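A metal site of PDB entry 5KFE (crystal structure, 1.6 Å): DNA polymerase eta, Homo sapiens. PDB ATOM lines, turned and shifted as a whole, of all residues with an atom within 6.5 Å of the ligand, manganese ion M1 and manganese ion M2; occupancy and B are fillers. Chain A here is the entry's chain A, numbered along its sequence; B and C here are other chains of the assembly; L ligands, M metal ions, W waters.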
ATOM      1  N   ASP A  16      -4.256 -39.736   3.349  1.00  0.00           N
ATOM      2  CA  ASP A  16      -5.001 -38.495   3.415  1.00  0.00           C
ATOM      3  C   ASP A  16      -6.429 -38.691   3.921  1.00  0.00           C
ATOM      4  O   ASP A  16      -7.110 -39.460   3.402  1.00  0.00           O
ATOM      5  CB  ASP A  16      -5.099 -37.882   2.045  1.00  0.00           C
ATOM      6  CG  ASP A  16      -5.730 -36.563   2.046  1.00  0.00           C
ATOM      7  OD1 ASP A  16      -6.861 -36.499   1.845  1.00  0.00           O
ATOM      8  OD2 ASP A  16      -5.014 -35.637   2.169  1.00  0.00           O
ATOM      9  N   MET A  17      -6.806 -37.956   4.932  1.00  0.00           N
ATOM     10  CA  MET A  17      -8.135 -38.190   5.517  1.00  0.00           C
ATOM     11  C   MET A  17      -9.271 -37.812   4.563  1.00  0.00           C
ATOM     12  O   MET A  17      -9.148 -36.858   3.813  1.00  0.00           O
ATOM     13  CB  MET A  17      -8.280 -37.392   6.827  1.00  0.00           C
ATOM     14  CG  MET A  17      -7.177 -37.657   7.825  1.00  0.00           C
ATOM     15  SD  MET A  17      -6.905 -39.403   8.204  1.00  0.00           S
ATOM     16  CE  MET A  17      -8.434 -39.821   8.971  1.00  0.00           C
ATOM     17  N   ASP A  18     -10.364 -38.551   4.546  1.00  0.00           N
ATOM     18  CA  ASP A  18     -11.497 -38.199   3.704  1.00  0.00           C
ATOM     19  C   ASP A  18     -12.258 -37.039   4.354  1.00  0.00           C
ATOM     20  O   ASP A  18     -12.500 -37.068   5.511  1.00  0.00           O
ATOM     21  CB  ASP A  18     -12.415 -39.389   3.539  1.00  0.00           C
ATOM     22  CG  ASP A  18     -11.762 -40.560   2.794  1.00  0.00           C
ATOM     23  OD1 ASP A  18     -10.808 -40.358   2.075  1.00  0.00           O
ATOM     24  OD2 ASP A  18     -12.252 -41.612   2.937  1.00  0.00           O
ATOM     25  N   CYS A  19     -12.604 -36.048   3.542  1.00  0.00           N
ATOM     26  CA  CYS A  19     -13.357 -34.845   3.953  1.00  0.00           C
ATOM     27  C   CYS A  19     -13.140 -34.561   5.450  1.00  0.00           C
ATOM     28  O   CYS A  19     -14.075 -34.608   6.255  1.00  0.00           O
ATOM     29  CB  CYS A  19     -14.855 -34.966   3.623  1.00  0.00           C
ATOM     30  SG  CYS A  19     -15.753 -36.438   4.143  1.00  0.00           S
ATOM     31  N   PHE A  20     -11.889 -34.277   5.815  1.00  0.00           N
ATOM     32  CA  PHE A  20     -11.438 -34.393   7.198  1.00  0.00           C
ATOM     33  C   PHE A  20     -12.258 -33.608   8.225  1.00  0.00           C
ATOM     34  O   PHE A  20     -12.750 -34.199   9.184  1.00  0.00           O
ATOM     35  CB  PHE A  20      -9.957 -33.995   7.319  1.00  0.00           C
ATOM     36  CG  PHE A  20      -9.385 -34.219   8.698  1.00  0.00           C
ATOM     37  CD1 PHE A  20      -9.642 -35.393   9.383  1.00  0.00           C
ATOM     38  CD2 PHE A  20      -8.581 -33.248   9.287  1.00  0.00           C
ATOM     39  CE1 PHE A  20      -9.087 -35.598  10.665  1.00  0.00           C
ATOM     40  CE2 PHE A  20      -8.028 -33.463  10.554  1.00  0.00           C
ATOM     41  CZ  PHE A  20      -8.284 -34.627  11.240  1.00  0.00           C
ATOM     42  N   PHE A  21     -12.399 -32.296   8.048  1.00  0.00           N
ATOM     43  CA  PHE A  21     -13.096 -31.508   9.077  1.00  0.00           C
ATOM     44  C   PHE A  21     -14.545 -31.985   9.220  1.00  0.00           C
ATOM     45  O   PHE A  21     -15.117 -31.935  10.305  1.00  0.00           O
ATOM     46  CB  PHE A  21     -13.067 -30.000   8.783  1.00  0.00           C
ATOM     47  CG  PHE A  21     -11.727 -29.343   8.947  1.00  0.00           C
ATOM     48  CD1 PHE A  21     -10.539 -30.068   9.070  1.00  0.00           C
ATOM     49  CD2 PHE A  21     -11.656 -27.959   8.956  1.00  0.00           C
ATOM     50  CE1 PHE A  21      -9.307 -29.405   9.203  1.00  0.00           C
ATOM     51  CE2 PHE A  21     -10.438 -27.294   9.104  1.00  0.00           C
ATOM     52  CZ  PHE A  21      -9.264 -28.017   9.213  1.00  0.00           C
ATOM     53  N   VAL A  22     -15.161 -32.407   8.102  1.00  0.00           N
ATOM     54  CA  VAL A  22     -16.510 -32.953   8.165  1.00  0.00           C
ATOM     55  C   VAL A  22     -16.535 -34.229   9.012  1.00  0.00           C
ATOM     56  O   VAL A  22     -17.425 -34.385   9.865  1.00  0.00           O
ATOM     57  CB  VAL A  22     -17.051 -33.238   6.755  1.00  0.00           C
ATOM     58  CG1 VAL A  22     -18.286 -34.153   6.798  1.00  0.00           C
ATOM     59  CG2 VAL A  22     -17.371 -31.922   6.025  1.00  0.00           C
ATOM     60  N   GLN A  41     -16.929 -21.507   8.020  1.00  0.00           N
ATOM     61  CA  GLN A  41     -16.387 -20.562   8.982  1.00  0.00           C
ATOM     62  C   GLN A  41     -17.067 -19.215   8.788  1.00  0.00           C
ATOM     63  O   GLN A  41     -17.282 -18.772   7.662  1.00  0.00           O
ATOM     64  CB  GLN A  41     -14.868 -20.442   8.899  1.00  0.00           C
ATOM     65  CG  GLN A  41     -14.301 -20.203   7.534  1.00  0.00           C
ATOM     66  CD  GLN A  41     -12.791 -20.388   7.518  1.00  0.00           C
ATOM     67  OE1 GLN A  41     -12.201 -20.895   8.475  1.00  0.00           O
ATOM     68  NE2 GLN A  41     -12.164 -19.971   6.437  1.00  0.00           N
ATOM     69  N   ILE A  51     -15.338 -24.794   4.008  1.00  0.00           N
ATOM     70  CA  ILE A  51     -13.954 -25.251   3.925  1.00  0.00           C
ATOM     71  C   ILE A  51     -13.827 -26.781   3.849  1.00  0.00           C
ATOM     72  O   ILE A  51     -12.744 -27.289   3.592  1.00  0.00           O
ATOM     73  CB  ILE A  51     -13.101 -24.745   5.115  1.00  0.00           C
ATOM     74  CG1 ILE A  51     -13.676 -25.193   6.461  1.00  0.00           C
ATOM     75  CG2 ILE A  51     -12.979 -23.211   5.039  1.00  0.00           C
ATOM     76  CD1 ILE A  51     -12.758 -24.836   7.640  1.00  0.00           C
ATOM     77  N   ALA A  52     -14.923 -27.520   4.031  1.00  0.00           N
ATOM     78  CA  ALA A  52     -14.891 -28.982   3.878  1.00  0.00           C
ATOM     79  C   ALA A  52     -16.285 -29.490   3.534  1.00  0.00           C
ATOM     80  O   ALA A  52     -17.277 -28.925   4.003  1.00  0.00           O
ATOM     81  CB  ALA A  52     -14.358 -29.669   5.160  1.00  0.00           C
ATOM     82  N   VAL A  53     -16.361 -30.537   2.716  1.00  0.00           N
ATOM     83  CA  VAL A  53     -17.624 -30.990   2.136  1.00  0.00           C
ATOM     84  C   VAL A  53     -17.714 -32.514   2.134  1.00  0.00           C
ATOM     85  O   VAL A  53     -16.800 -33.167   1.614  1.00  0.00           O
ATOM     86  CB  VAL A  53     -17.779 -30.496   0.669  1.00  0.00           C
ATOM     87  CG1 VAL A  53     -19.163 -30.804   0.132  1.00  0.00           C
ATOM     88  CG2 VAL A  53     -17.494 -29.013   0.554  1.00  0.00           C
ATOM     89  N   TYR A  55     -18.951 -36.286   0.984  1.00  0.00           N
ATOM     90  CA  TYR A  55     -19.093 -36.810  -0.374  1.00  0.00           C
ATOM     91  C   TYR A  55     -20.553 -36.808  -0.826  1.00  0.00           C
ATOM     92  O   TYR A  55     -20.831 -36.606  -2.006  1.00  0.00           O
ATOM     93  CB  TYR A  55     -18.455 -38.196  -0.471  1.00  0.00           C
ATOM     94  CG  TYR A  55     -16.951 -38.061  -0.595  1.00  0.00           C
ATOM     95  CD1 TYR A  55     -16.155 -37.846   0.524  1.00  0.00           C
ATOM     96  CD2 TYR A  55     -16.346 -38.066  -1.842  1.00  0.00           C
ATOM     97  CE1 TYR A  55     -14.795 -37.672   0.416  1.00  0.00           C
ATOM     98  CE2 TYR A  55     -14.979 -37.893  -1.971  1.00  0.00           C
ATOM     99  CZ  TYR A  55     -14.207 -37.695  -0.845  1.00  0.00           C
ATOM    100  OH  TYR A  55     -12.850 -37.529  -0.996  1.00  0.00           O
ATOM    101  N   ARG A  58     -20.990 -33.325  -2.093  1.00  0.00           N
ATOM    102  CA  ARG A  58     -20.285 -33.110  -3.360  1.00  0.00           C
ATOM    103  C   ARG A  58     -21.116 -33.559  -4.562  1.00  0.00           C
ATOM    104  O   ARG A  58     -20.990 -32.982  -5.646  1.00  0.00           O
ATOM    105  CB  ARG A  58     -18.940 -33.840  -3.365  1.00  0.00           C
ATOM    106  CG  ARG A  58     -18.013 -33.367  -2.293  1.00  0.00           C
ATOM    107  CD  ARG A  58     -16.673 -34.051  -2.373  1.00  0.00           C
ATOM    108  NE  ARG A  58     -15.953 -33.813  -1.122  1.00  0.00           N
ATOM    109  CZ  ARG A  58     -14.664 -34.080  -0.927  1.00  0.00           C
ATOM    110  NH1 ARG A  58     -13.925 -34.573  -1.912  1.00  0.00           N
ATOM    111  NH2 ARG A  58     -14.115 -33.816   0.277  1.00  0.00           N
ATOM    112  N   ARG A  64     -15.569 -26.647  -1.716  1.00  0.00           N
ATOM    113  CA  ARG A  64     -14.801 -25.714  -0.915  1.00  0.00           C
ATOM    114  C   ARG A  64     -14.809 -24.332  -1.583  1.00  0.00           C
ATOM    115  O   ARG A  64     -14.905 -24.243  -2.808  1.00  0.00           O
ATOM    116  CB  ARG A  64     -13.372 -26.262  -0.736  1.00  0.00           C
ATOM    117  CG  ARG A  64     -12.335 -25.290  -0.206  1.00  0.00           C
ATOM    118  CD  ARG A  64     -11.030 -26.048   0.037  1.00  0.00           C
ATOM    119  NE  ARG A  64     -11.283 -27.097   1.013  1.00  0.00           N
ATOM    120  CZ  ARG A  64     -10.918 -28.373   0.892  1.00  0.00           C
ATOM    121  NH1 ARG A  64     -10.247 -28.812  -0.171  1.00  0.00           N
ATOM    122  NH2 ARG A  64     -11.231 -29.231   1.854  1.00  0.00           N
ATOM    123  N   LEU A  92      -9.041 -23.243  14.971  1.00  0.00           N
ATOM    124  CA  LEU A  92      -8.995 -24.582  14.378  1.00  0.00           C
ATOM    125  C   LEU A  92      -8.499 -25.681  15.318  1.00  0.00           C
ATOM    126  O   LEU A  92      -8.132 -26.768  14.875  1.00  0.00           O
ATOM    127  CB  LEU A  92      -8.122 -24.552  13.114  1.00  0.00           C
ATOM    128  CG  LEU A  92      -8.508 -23.465  12.112  1.00  0.00           C
ATOM    129  CD1 LEU A  92      -7.506 -23.429  10.977  1.00  0.00           C
ATOM    130  CD2 LEU A  92      -9.921 -23.729  11.599  1.00  0.00           C
ATOM    131  N   SER A 116       0.279 -31.968   5.817  1.00  0.00           N
ATOM    132  CA  SER A 116      -0.812 -31.021   6.022  1.00  0.00           C
ATOM    133  C   SER A 116      -1.539 -31.406   7.308  1.00  0.00           C
ATOM    134  O   SER A 116      -1.177 -32.379   7.956  1.00  0.00           O
ATOM    135  CB  SER A 116      -1.803 -31.025   4.861  1.00  0.00           C
ATOM    136  OG  SER A 116      -2.721 -32.109   4.972  1.00  0.00           O
ATOM    137  N   ILE A 117      -2.595 -30.673   7.640  1.00  0.00           N
ATOM    138  CA  ILE A 117      -3.358 -31.026   8.824  1.00  0.00           C
ATOM    139  C   ILE A 117      -4.008 -32.416   8.684  1.00  0.00           C
ATOM    140  O   ILE A 117      -4.348 -33.049   9.676  1.00  0.00           O
ATOM    141  CB  ILE A 117      -4.439 -29.934   9.108  1.00  0.00           C
ATOM    142  CG1 ILE A 117      -4.935 -30.044  10.542  1.00  0.00           C
ATOM    143  CG2 ILE A 117      -5.578 -30.026   8.090  1.00  0.00           C
ATOM    144  CD1 ILE A 117      -5.739 -28.806  10.986  1.00  0.00           C
ATOM    145  N   ASP A 118      -4.183 -32.912   7.457  1.00  0.00           N
ATOM    146  CA  ASP A 118      -4.889 -34.182   7.313  1.00  0.00           C
ATOM    147  C   ASP A 118      -4.159 -35.239   6.494  1.00  0.00           C
ATOM    148  O   ASP A 118      -4.770 -36.213   6.051  1.00  0.00           O
ATOM    149  CB  ASP A 118      -6.291 -33.958   6.709  1.00  0.00           C
ATOM    150  CG  ASP A 118      -6.303 -34.026   5.181  1.00  0.00           C
ATOM    151  OD1 ASP A 118      -5.384 -33.508   4.490  1.00  0.00           O
ATOM    152  OD2 ASP A 118      -7.254 -34.687   4.667  1.00  0.00           O
ATOM    153  N   GLU A 119      -2.848 -35.073   6.289  1.00  0.00           N
ATOM    154  CA  GLU A 119      -2.116 -36.083   5.536  1.00  0.00           C
ATOM    155  C   GLU A 119      -0.659 -36.180   5.897  1.00  0.00           C
ATOM    156  O   GLU A 119      -0.047 -35.207   6.367  1.00  0.00           O
ATOM    157  CB  GLU A 119      -2.241 -35.833   4.032  1.00  0.00           C
ATOM    158  CG  GLU A 119      -1.394 -34.687   3.502  1.00  0.00           C
ATOM    159  CD  GLU A 119      -2.040 -34.068   2.285  1.00  0.00           C
ATOM    160  OE1 GLU A 119      -1.619 -34.368   1.149  1.00  0.00           O
ATOM    161  OE2 GLU A 119      -3.006 -33.299   2.467  1.00  0.00           O
ATOM    162  N   SER A 216      -8.028 -42.235   2.660  1.00  0.00           N
ATOM    163  CA  SER A 216      -7.565 -42.880   1.437  1.00  0.00           C
ATOM    164  C   SER A 216      -6.058 -42.895   1.461  1.00  0.00           C
ATOM    165  O   SER A 216      -5.455 -42.244   2.295  1.00  0.00           O
ATOM    166  CB  SER A 216      -8.094 -42.136   0.222  1.00  0.00           C
ATOM    167  OG  SER A 216      -9.517 -42.193   0.212  1.00  0.00           O
ATOM    168  N   LYS A 227       1.147 -39.376  -3.708  1.00  0.00           N
ATOM    169  CA  LYS A 227       0.103 -38.360  -3.600  1.00  0.00           C
ATOM    170  C   LYS A 227      -0.895 -38.464  -4.760  1.00  0.00           C
ATOM    171  O   LYS A 227      -2.102 -38.392  -4.545  1.00  0.00           O
ATOM    172  CB  LYS A 227       0.729 -36.952  -3.565  1.00  0.00           C
ATOM    173  CG  LYS A 227      -0.313 -35.830  -3.543  1.00  0.00           C
ATOM    174  CD  LYS A 227      -1.234 -35.881  -2.320  1.00  0.00           C
ATOM    175  CE  LYS A 227      -2.213 -34.705  -2.341  1.00  0.00           C
ATOM    176  NZ  LYS A 227      -3.084 -34.591  -1.124  1.00  0.00           N
ATOM    177  N   LYS A 234     -10.566 -42.107  -4.160  1.00  0.00           N
ATOM    178  CA  LYS A 234     -11.248 -41.656  -2.932  1.00  0.00           C
ATOM    179  C   LYS A 234     -12.782 -41.714  -3.030  1.00  0.00           C
ATOM    180  O   LYS A 234     -13.269 -41.570  -4.084  1.00  0.00           O
ATOM    181  CB  LYS A 234     -10.728 -40.271  -2.561  1.00  0.00           C
ATOM    182  CG  LYS A 234     -10.761 -39.327  -3.680  1.00  0.00           C
ATOM    183  CD  LYS A 234     -10.187 -37.971  -3.284  1.00  0.00           C
ATOM    184  CE  LYS A 234     -11.110 -36.841  -3.734  1.00  0.00           C
ATOM    185  NZ  LYS A 234     -10.456 -35.553  -3.396  1.00  0.00           N
ATOM    186  N   PRO A 235     -13.520 -41.844  -1.934  1.00  0.00           N
ATOM    187  CA  PRO A 235     -12.999 -41.958  -0.567  1.00  0.00           C
ATOM    188  C   PRO A 235     -12.852 -43.398  -0.107  1.00  0.00           C
ATOM    189  O   PRO A 235     -13.334 -44.327  -0.772  1.00  0.00           O
ATOM    190  CB  PRO A 235     -14.084 -41.268   0.254  1.00  0.00           C
ATOM    191  CG  PRO A 235     -15.354 -41.662  -0.472  1.00  0.00           C
ATOM    192  CD  PRO A 235     -14.984 -41.724  -1.953  1.00  0.00           C
ATOM    193  P    DT B   8      -2.912 -29.569  -2.476  1.00  0.00           P
ATOM    194  OP1  DT B   8      -3.016 -31.000  -2.848  1.00  0.00           O
ATOM    195  OP2  DT B   8      -3.805 -28.563  -3.120  1.00  0.00           O
ATOM    196  O5'  DT B   8      -3.110 -29.385  -0.889  1.00  0.00           O
ATOM    197  C5'  DT B   8      -2.479 -30.254   0.144  1.00  0.00           C
ATOM    198  C4'  DT B   8      -3.154 -29.951   1.469  1.00  0.00           C
ATOM    199  O4'  DT B   8      -3.077 -28.512   1.587  1.00  0.00           O
ATOM    200  C3'  DT B   8      -4.637 -30.320   1.386  1.00  0.00           C
ATOM    201  O3'  DT B   8      -5.021 -31.087   2.534  1.00  0.00           O
ATOM    202  C2'  DT B   8      -5.358 -28.965   1.329  1.00  0.00           C
ATOM    203  C1'  DT B   8      -4.347 -28.004   1.944  1.00  0.00           C
ATOM    204  N1   DT B   8      -4.465 -26.606   1.445  1.00  0.00           N
ATOM    205  C2   DT B   8      -4.718 -25.600   2.346  1.00  0.00           C
ATOM    206  O2   DT B   8      -4.852 -25.787   3.533  1.00  0.00           O
ATOM    207  N3   DT B   8      -4.823 -24.342   1.788  1.00  0.00           N
ATOM    208  C4   DT B   8      -4.691 -24.006   0.470  1.00  0.00           C
ATOM    209  O4   DT B   8      -4.807 -22.847   0.069  1.00  0.00           O
ATOM    210  C5   DT B   8      -4.428 -25.106  -0.431  1.00  0.00           C
ATOM    211  C7   DT B   8      -4.266 -24.856  -1.905  1.00  0.00           C
ATOM    212  C6   DT B   8      -4.322 -26.341   0.100  1.00  0.00           C
ATOM    213  P    DT C   3     -14.567 -13.306  -2.748  1.00  0.00           P
ATOM    214  OP1  DT C   3     -13.588 -12.442  -3.435  1.00  0.00           O
ATOM    215  OP2  DT C   3     -15.804 -13.737  -3.427  1.00  0.00           O
ATOM    216  O5'  DT C   3     -13.801 -14.621  -2.237  1.00  0.00           O
ATOM    217  C5'  DT C   3     -14.420 -15.495  -1.319  1.00  0.00           C
ATOM    218  C4'  DT C   3     -13.420 -16.471  -0.756  1.00  0.00           C
ATOM    219  O4'  DT C   3     -13.192 -17.532  -1.716  1.00  0.00           O
ATOM    220  C3'  DT C   3     -12.050 -15.855  -0.454  1.00  0.00           C
ATOM    221  O3'  DT C   3     -11.738 -15.993   0.927  1.00  0.00           O
ATOM    222  C2'  DT C   3     -11.072 -16.628  -1.353  1.00  0.00           C
ATOM    223  C1'  DT C   3     -11.839 -17.900  -1.686  1.00  0.00           C
ATOM    224  N1   DT C   3     -11.487 -18.484  -2.999  1.00  0.00           N
ATOM    225  C2   DT C   3     -10.974 -19.754  -3.055  1.00  0.00           C
ATOM    226  O2   DT C   3     -10.791 -20.439  -2.062  1.00  0.00           O
ATOM    227  N3   DT C   3     -10.686 -20.200  -4.315  1.00  0.00           N
ATOM    228  C4   DT C   3     -10.863 -19.505  -5.506  1.00  0.00           C
ATOM    229  O4   DT C   3     -10.579 -19.991  -6.590  1.00  0.00           O
ATOM    230  C5   DT C   3     -11.407 -18.175  -5.373  1.00  0.00           C
ATOM    231  C7   DT C   3     -11.630 -17.331  -6.589  1.00  0.00           C
ATOM    232  C6   DT C   3     -11.689 -17.728  -4.135  1.00  0.00           C
ATOM    233  P    DT C   4     -11.527 -14.654   1.807  1.00  0.00           P
ATOM    234  OP1  DT C   4     -12.768 -13.875   1.753  1.00  0.00           O
ATOM    235  OP2  DT C   4     -10.250 -14.066   1.352  1.00  0.00           O
ATOM    236  O5'  DT C   4     -11.269 -15.194   3.301  1.00  0.00           O
ATOM    237  C5'  DT C   4     -12.361 -15.477   4.184  1.00  0.00           C
ATOM    238  C4'  DT C   4     -11.861 -16.365   5.328  1.00  0.00           C
ATOM    239  O4'  DT C   4     -11.446 -17.623   4.752  1.00  0.00           O
ATOM    240  C3'  DT C   4     -10.642 -15.812   6.051  1.00  0.00           C
ATOM    241  O3'  DT C   4     -10.728 -16.197   7.415  1.00  0.00           O
ATOM    242  C2'  DT C   4      -9.473 -16.509   5.333  1.00  0.00           C
ATOM    243  C1'  DT C   4     -10.083 -17.867   5.066  1.00  0.00           C
ATOM    244  N1   DT C   4      -9.531 -18.629   3.932  1.00  0.00           N
ATOM    245  C2   DT C   4      -9.454 -19.982   4.081  1.00  0.00           C
ATOM    246  O2   DT C   4      -9.754 -20.553   5.117  1.00  0.00           O
ATOM    247  N3   DT C   4      -8.979 -20.645   2.992  1.00  0.00           N
ATOM    248  C4   DT C   4      -8.615 -20.114   1.773  1.00  0.00           C
ATOM    249  O4   DT C   4      -8.208 -20.817   0.855  1.00  0.00           O
ATOM    250  C5   DT C   4      -8.743 -18.676   1.667  1.00  0.00           C
ATOM    251  C7   DT C   4      -8.366 -17.971   0.395  1.00  0.00           C
ATOM    252  C6   DT C   4      -9.217 -18.002   2.743  1.00  0.00           C
ATOM    253  P    DA C   5      -9.588 -15.783   8.466  1.00  0.00           P
ATOM    254  OP1  DA C   5     -10.270 -15.455   9.729  1.00  0.00           O
ATOM    255  OP2  DA C   5      -8.671 -14.812   7.824  1.00  0.00           O
ATOM    256  O5'  DA C   5      -8.756 -17.109   8.647  1.00  0.00           O
ATOM    257  C5'  DA C   5      -9.351 -18.235   9.294  1.00  0.00           C
ATOM    258  C4'  DA C   5      -8.332 -19.333   9.451  1.00  0.00           C
ATOM    259  O4'  DA C   5      -7.998 -19.895   8.148  1.00  0.00           O
ATOM    260  C3'  DA C   5      -7.011 -18.890  10.071  1.00  0.00           C
ATOM    261  O3'  DA C   5      -6.545 -19.909  10.925  1.00  0.00           O
ATOM    262  C2'  DA C   5      -6.110 -18.715   8.850  1.00  0.00           C
ATOM    263  C1'  DA C   5      -6.598 -19.886   7.993  1.00  0.00           C
ATOM    264  N9   DA C   5      -6.304 -19.748   6.577  1.00  0.00           N
ATOM    265  C8   DA C   5      -6.290 -18.599   5.837  1.00  0.00           C
ATOM    266  N7   DA C   5      -6.027 -18.799   4.565  1.00  0.00           N
ATOM    267  C5   DA C   5      -5.851 -20.172   4.468  1.00  0.00           C
ATOM    268  C6   DA C   5      -5.536 -21.015   3.382  1.00  0.00           C
ATOM    269  N6   DA C   5      -5.341 -20.561   2.138  1.00  0.00           N
ATOM    270  N1   DA C   5      -5.435 -22.336   3.631  1.00  0.00           N
ATOM    271  C2   DA C   5      -5.643 -22.779   4.876  1.00  0.00           C
ATOM    272  N3   DA C   5      -5.934 -22.082   5.981  1.00  0.00           N
ATOM    273  C4   DA C   5      -6.030 -20.769   5.695  1.00  0.00           C
HETATM  274  P1  LIG L   1     -10.817 -35.058   0.529  1.00  0.00           P
HETATM  275  O1  LIG L   1     -11.040 -34.656  -0.926  1.00  0.00           O
HETATM  276  O2  LIG L   1     -11.546 -36.322   0.876  1.00  0.00           O
HETATM  277  O3  LIG L   1      -9.348 -35.155   0.847  1.00  0.00           O
HETATM  278  P2  LIG L   1     -10.708 -32.996   2.491  1.00  0.00           P
HETATM  279  O4  LIG L   1      -9.994 -33.876   3.505  1.00  0.00           O
HETATM  280  O5  LIG L   1     -11.724 -32.083   3.131  1.00  0.00           O
HETATM  281  O6  LIG L   1     -11.473 -33.904   1.408  1.00  0.00           O
HETATM  282  P3  LIG L   1      -8.159 -31.807   1.902  1.00  0.00           P
HETATM  283  O7  LIG L   1      -7.720 -30.993   0.704  1.00  0.00           O
HETATM  284  O8  LIG L   1      -7.345 -33.060   2.088  1.00  0.00           O
HETATM  285  O9  LIG L   1      -9.705 -32.107   1.649  1.00  0.00           O
HETATM  286  O10 LIG L   1      -8.074 -30.876   3.167  1.00  0.00           O
HETATM  287  C1  LIG L   1      -8.113 -31.366   4.486  1.00  0.00           C
HETATM  288  C2  LIG L   1      -8.801 -30.372   5.428  1.00  0.00           C
HETATM  289  O11 LIG L   1      -8.036 -29.193   5.429  1.00  0.00           O
HETATM  290  C3  LIG L   1     -10.148 -30.013   4.985  1.00  0.00           C
HETATM  291  O12 LIG L   1     -11.141 -30.878   5.552  1.00  0.00           O
HETATM  292  C4  LIG L   1     -10.332 -28.638   5.452  1.00  0.00           C
HETATM  293  C5  LIG L   1      -8.938 -28.079   5.415  1.00  0.00           C
HETATM  294  N1  LIG L   1      -8.701 -27.291   4.254  1.00  0.00           N
HETATM  295  C6  LIG L   1      -8.325 -27.730   3.019  1.00  0.00           C
HETATM  296  N2  LIG L   1      -8.191 -26.713   2.181  1.00  0.00           N
HETATM  297  C7  LIG L   1      -8.447 -25.582   2.842  1.00  0.00           C
HETATM  298  C8  LIG L   1      -8.463 -24.227   2.505  1.00  0.00           C
HETATM  299  N3  LIG L   1      -8.159 -23.833   1.175  1.00  0.00           N
HETATM  300  N4  LIG L   1      -8.785 -23.323   3.432  1.00  0.00           N
HETATM  301  C9  LIG L   1      -9.092 -23.663   4.702  1.00  0.00           C
HETATM  302  N5  LIG L   1      -9.077 -24.979   5.076  1.00  0.00           N
HETATM  303  C10 LIG L   1      -8.766 -25.923   4.169  1.00  0.00           C
HETATM  304 MN    MN M   1      -5.147 -33.405   2.365  1.00  0.00          MN
HETATM  305 MN    MN M   2      -8.285 -35.105   2.851  1.00  0.00          MN
HETATM  306  O   HOH W   1      -7.666 -26.370  -0.645  1.00  0.00           O
HETATM  307  O   HOH W   2      -5.190 -33.243   0.214  1.00  0.00           O
HETATM  308  O   HOH W   3     -13.846 -31.301   1.692  1.00  0.00           O
HETATM  309  O   HOH W   4      -7.378 -34.671  -0.943  1.00  0.00           O
HETATM  310  O   HOH W   5     -11.179 -32.209  -1.908  1.00  0.00           O
HETATM  311  O   HOH W   6      -8.770 -24.685   7.838  1.00  0.00           O
HETATM  312  O   HOH W   7      -5.281 -29.638   4.625  1.00  0.00           O
HETATM  313  O   HOH W   8      -5.766 -26.654   6.003  1.00  0.00           O
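The side-chain carboxylate (OD2) of Asp 118 is bound to manganese ion M2.
O of Met 17 is bound to manganese ion M2 (2.2 Å).
An oxygen (O4) of the ligand is bound to manganese ion M2, at 2.2 Å.
OD1 of Asp 16 binds manganese ion M2 (2.2 Å).
O3 of the ligand binds manganese ion M2, at 2.3 Å.
Manganese ion M2 is bound by O8 of the ligand (2.4 Å).
Manganese ion M2 has six donor atoms within binding distance.
Ser 116 touches manganese ion M1.
Of the 27 residues printed, 5 come within 4 Å of manganese ion M1.
Along chain A the residues within 4 Å of manganese ion M1 span positions 16 to 119.
N3 of the ligand sits at hydrogen-bond distance from N3 of DT 8 of chain B (3.4 Å).
The side-chain hydroxyl (OH) of Tyr 55 sits at hydrogen-bond distance from an oxygen (O2) of the ligand.
The side-chain amino group (NZ) of Lys 234 is in salt-bridge range of an oxygen (O1) of the ligand (2.7 Å).
O4 of DT 4 of chain C is in hydrogen-bond range of a nitrogen (N3) of the ligand, 3.0 Å away.
The guanidinium group of Arg 58 is in salt-bridge range of an oxygen (O1) of the ligand.
The backbone NH (N) of Cys 19 lies within hydrogen-bond range of an oxygen (O2) of the ligand, 2.9 Å away.
The backbone NH of Phe 20 is in hydrogen-bond range of an oxygen (O5) of the ligand (3.5 Å).
N of Phe 21 lies within hydrogen-bond range of O12 of the ligand.
O5 of the ligand is in salt-bridge range of NH2 of Arg 64 (3.2 Å).
The side-chain hydroxyl (OG) of Ser 116 is in hydrogen-bond range of the backbone NH (N) of Asp 118.
The backbone NH (N) of Glu 119 lies within hydrogen-bond range of the side-chain hydroxyl (OG) of Ser 116, at 3.2 Å.
OE1 of Glu 119 is in salt-bridge range of NZ of Lys 227 (2.7 Å).
The side-chain amino group of Lys 227 lies close to the side-chain carboxylate of Asp 16 (3.96 Å).
O of Ser 216 is in hydrogen-bond range of N of Asp 16 (3.0 Å).
OP1 of DT 8 of chain B lies within salt-bridge range of NZ of Lys 227 (3.98 Å).
O2 of DT 4 of chain C sits at hydrogen-bond distance from the side-chain amide nitrogen (NE2) of Gln 41, 2.8 Å away.
The backbone carbonyl oxygen (O) of Val 53 sits at hydrogen-bond distance from the guanidinium group (NE) of Arg 58.
OD1 of Asp 118 is bound to manganese ion M1 (2.1 Å).
The side-chain carboxylate (OE2) of Glu 119 is bound to manganese ion M1 (2.1 Å).
Manganese ion M1 is bound by water W2, 2.2 Å away.
O8 of the ligand binds manganese ion M1 (2.2 Å).
OD2 of Asp 16 is bound to manganese ion M1.
O3' of DT 8 of chain B binds manganese ion M1 (2.3 Å).
Manganese ion M1 has six donor atoms within binding distance.
A nitrogen (N4) of the ligand sits close to N1 of DA 5 of chain C (3.5 Å).
CA of Asp 18 touches O2 of the ligand, 3.4 Å away.
Ile 51 touches the ligand.
Ala 52 touches the ligand.
Ile 117 touches the ligand (CG2 to O11, 3.7 Å).
Hydrophobic or aromatic side chains within 4 Å of the ligand: Phe 20, Phe 21, Ile 51, Ala 52, Tyr 55 and Ile 117.
Of the 27 residues printed, 17 come within 4 Å of the ligand.
The nearest printed residue that does not touch the ligand is Glu 119 (4.4 Å).
Water W2 lies within hydrogen-bond range of NZ of Lys 227 (2.8 Å) and O7 of the ligand (3.4 Å).
Water W8 bridges O2 of DT 8 of chain B (2.8 Å) and an oxygen (O11) of the ligand (3.5 Å).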
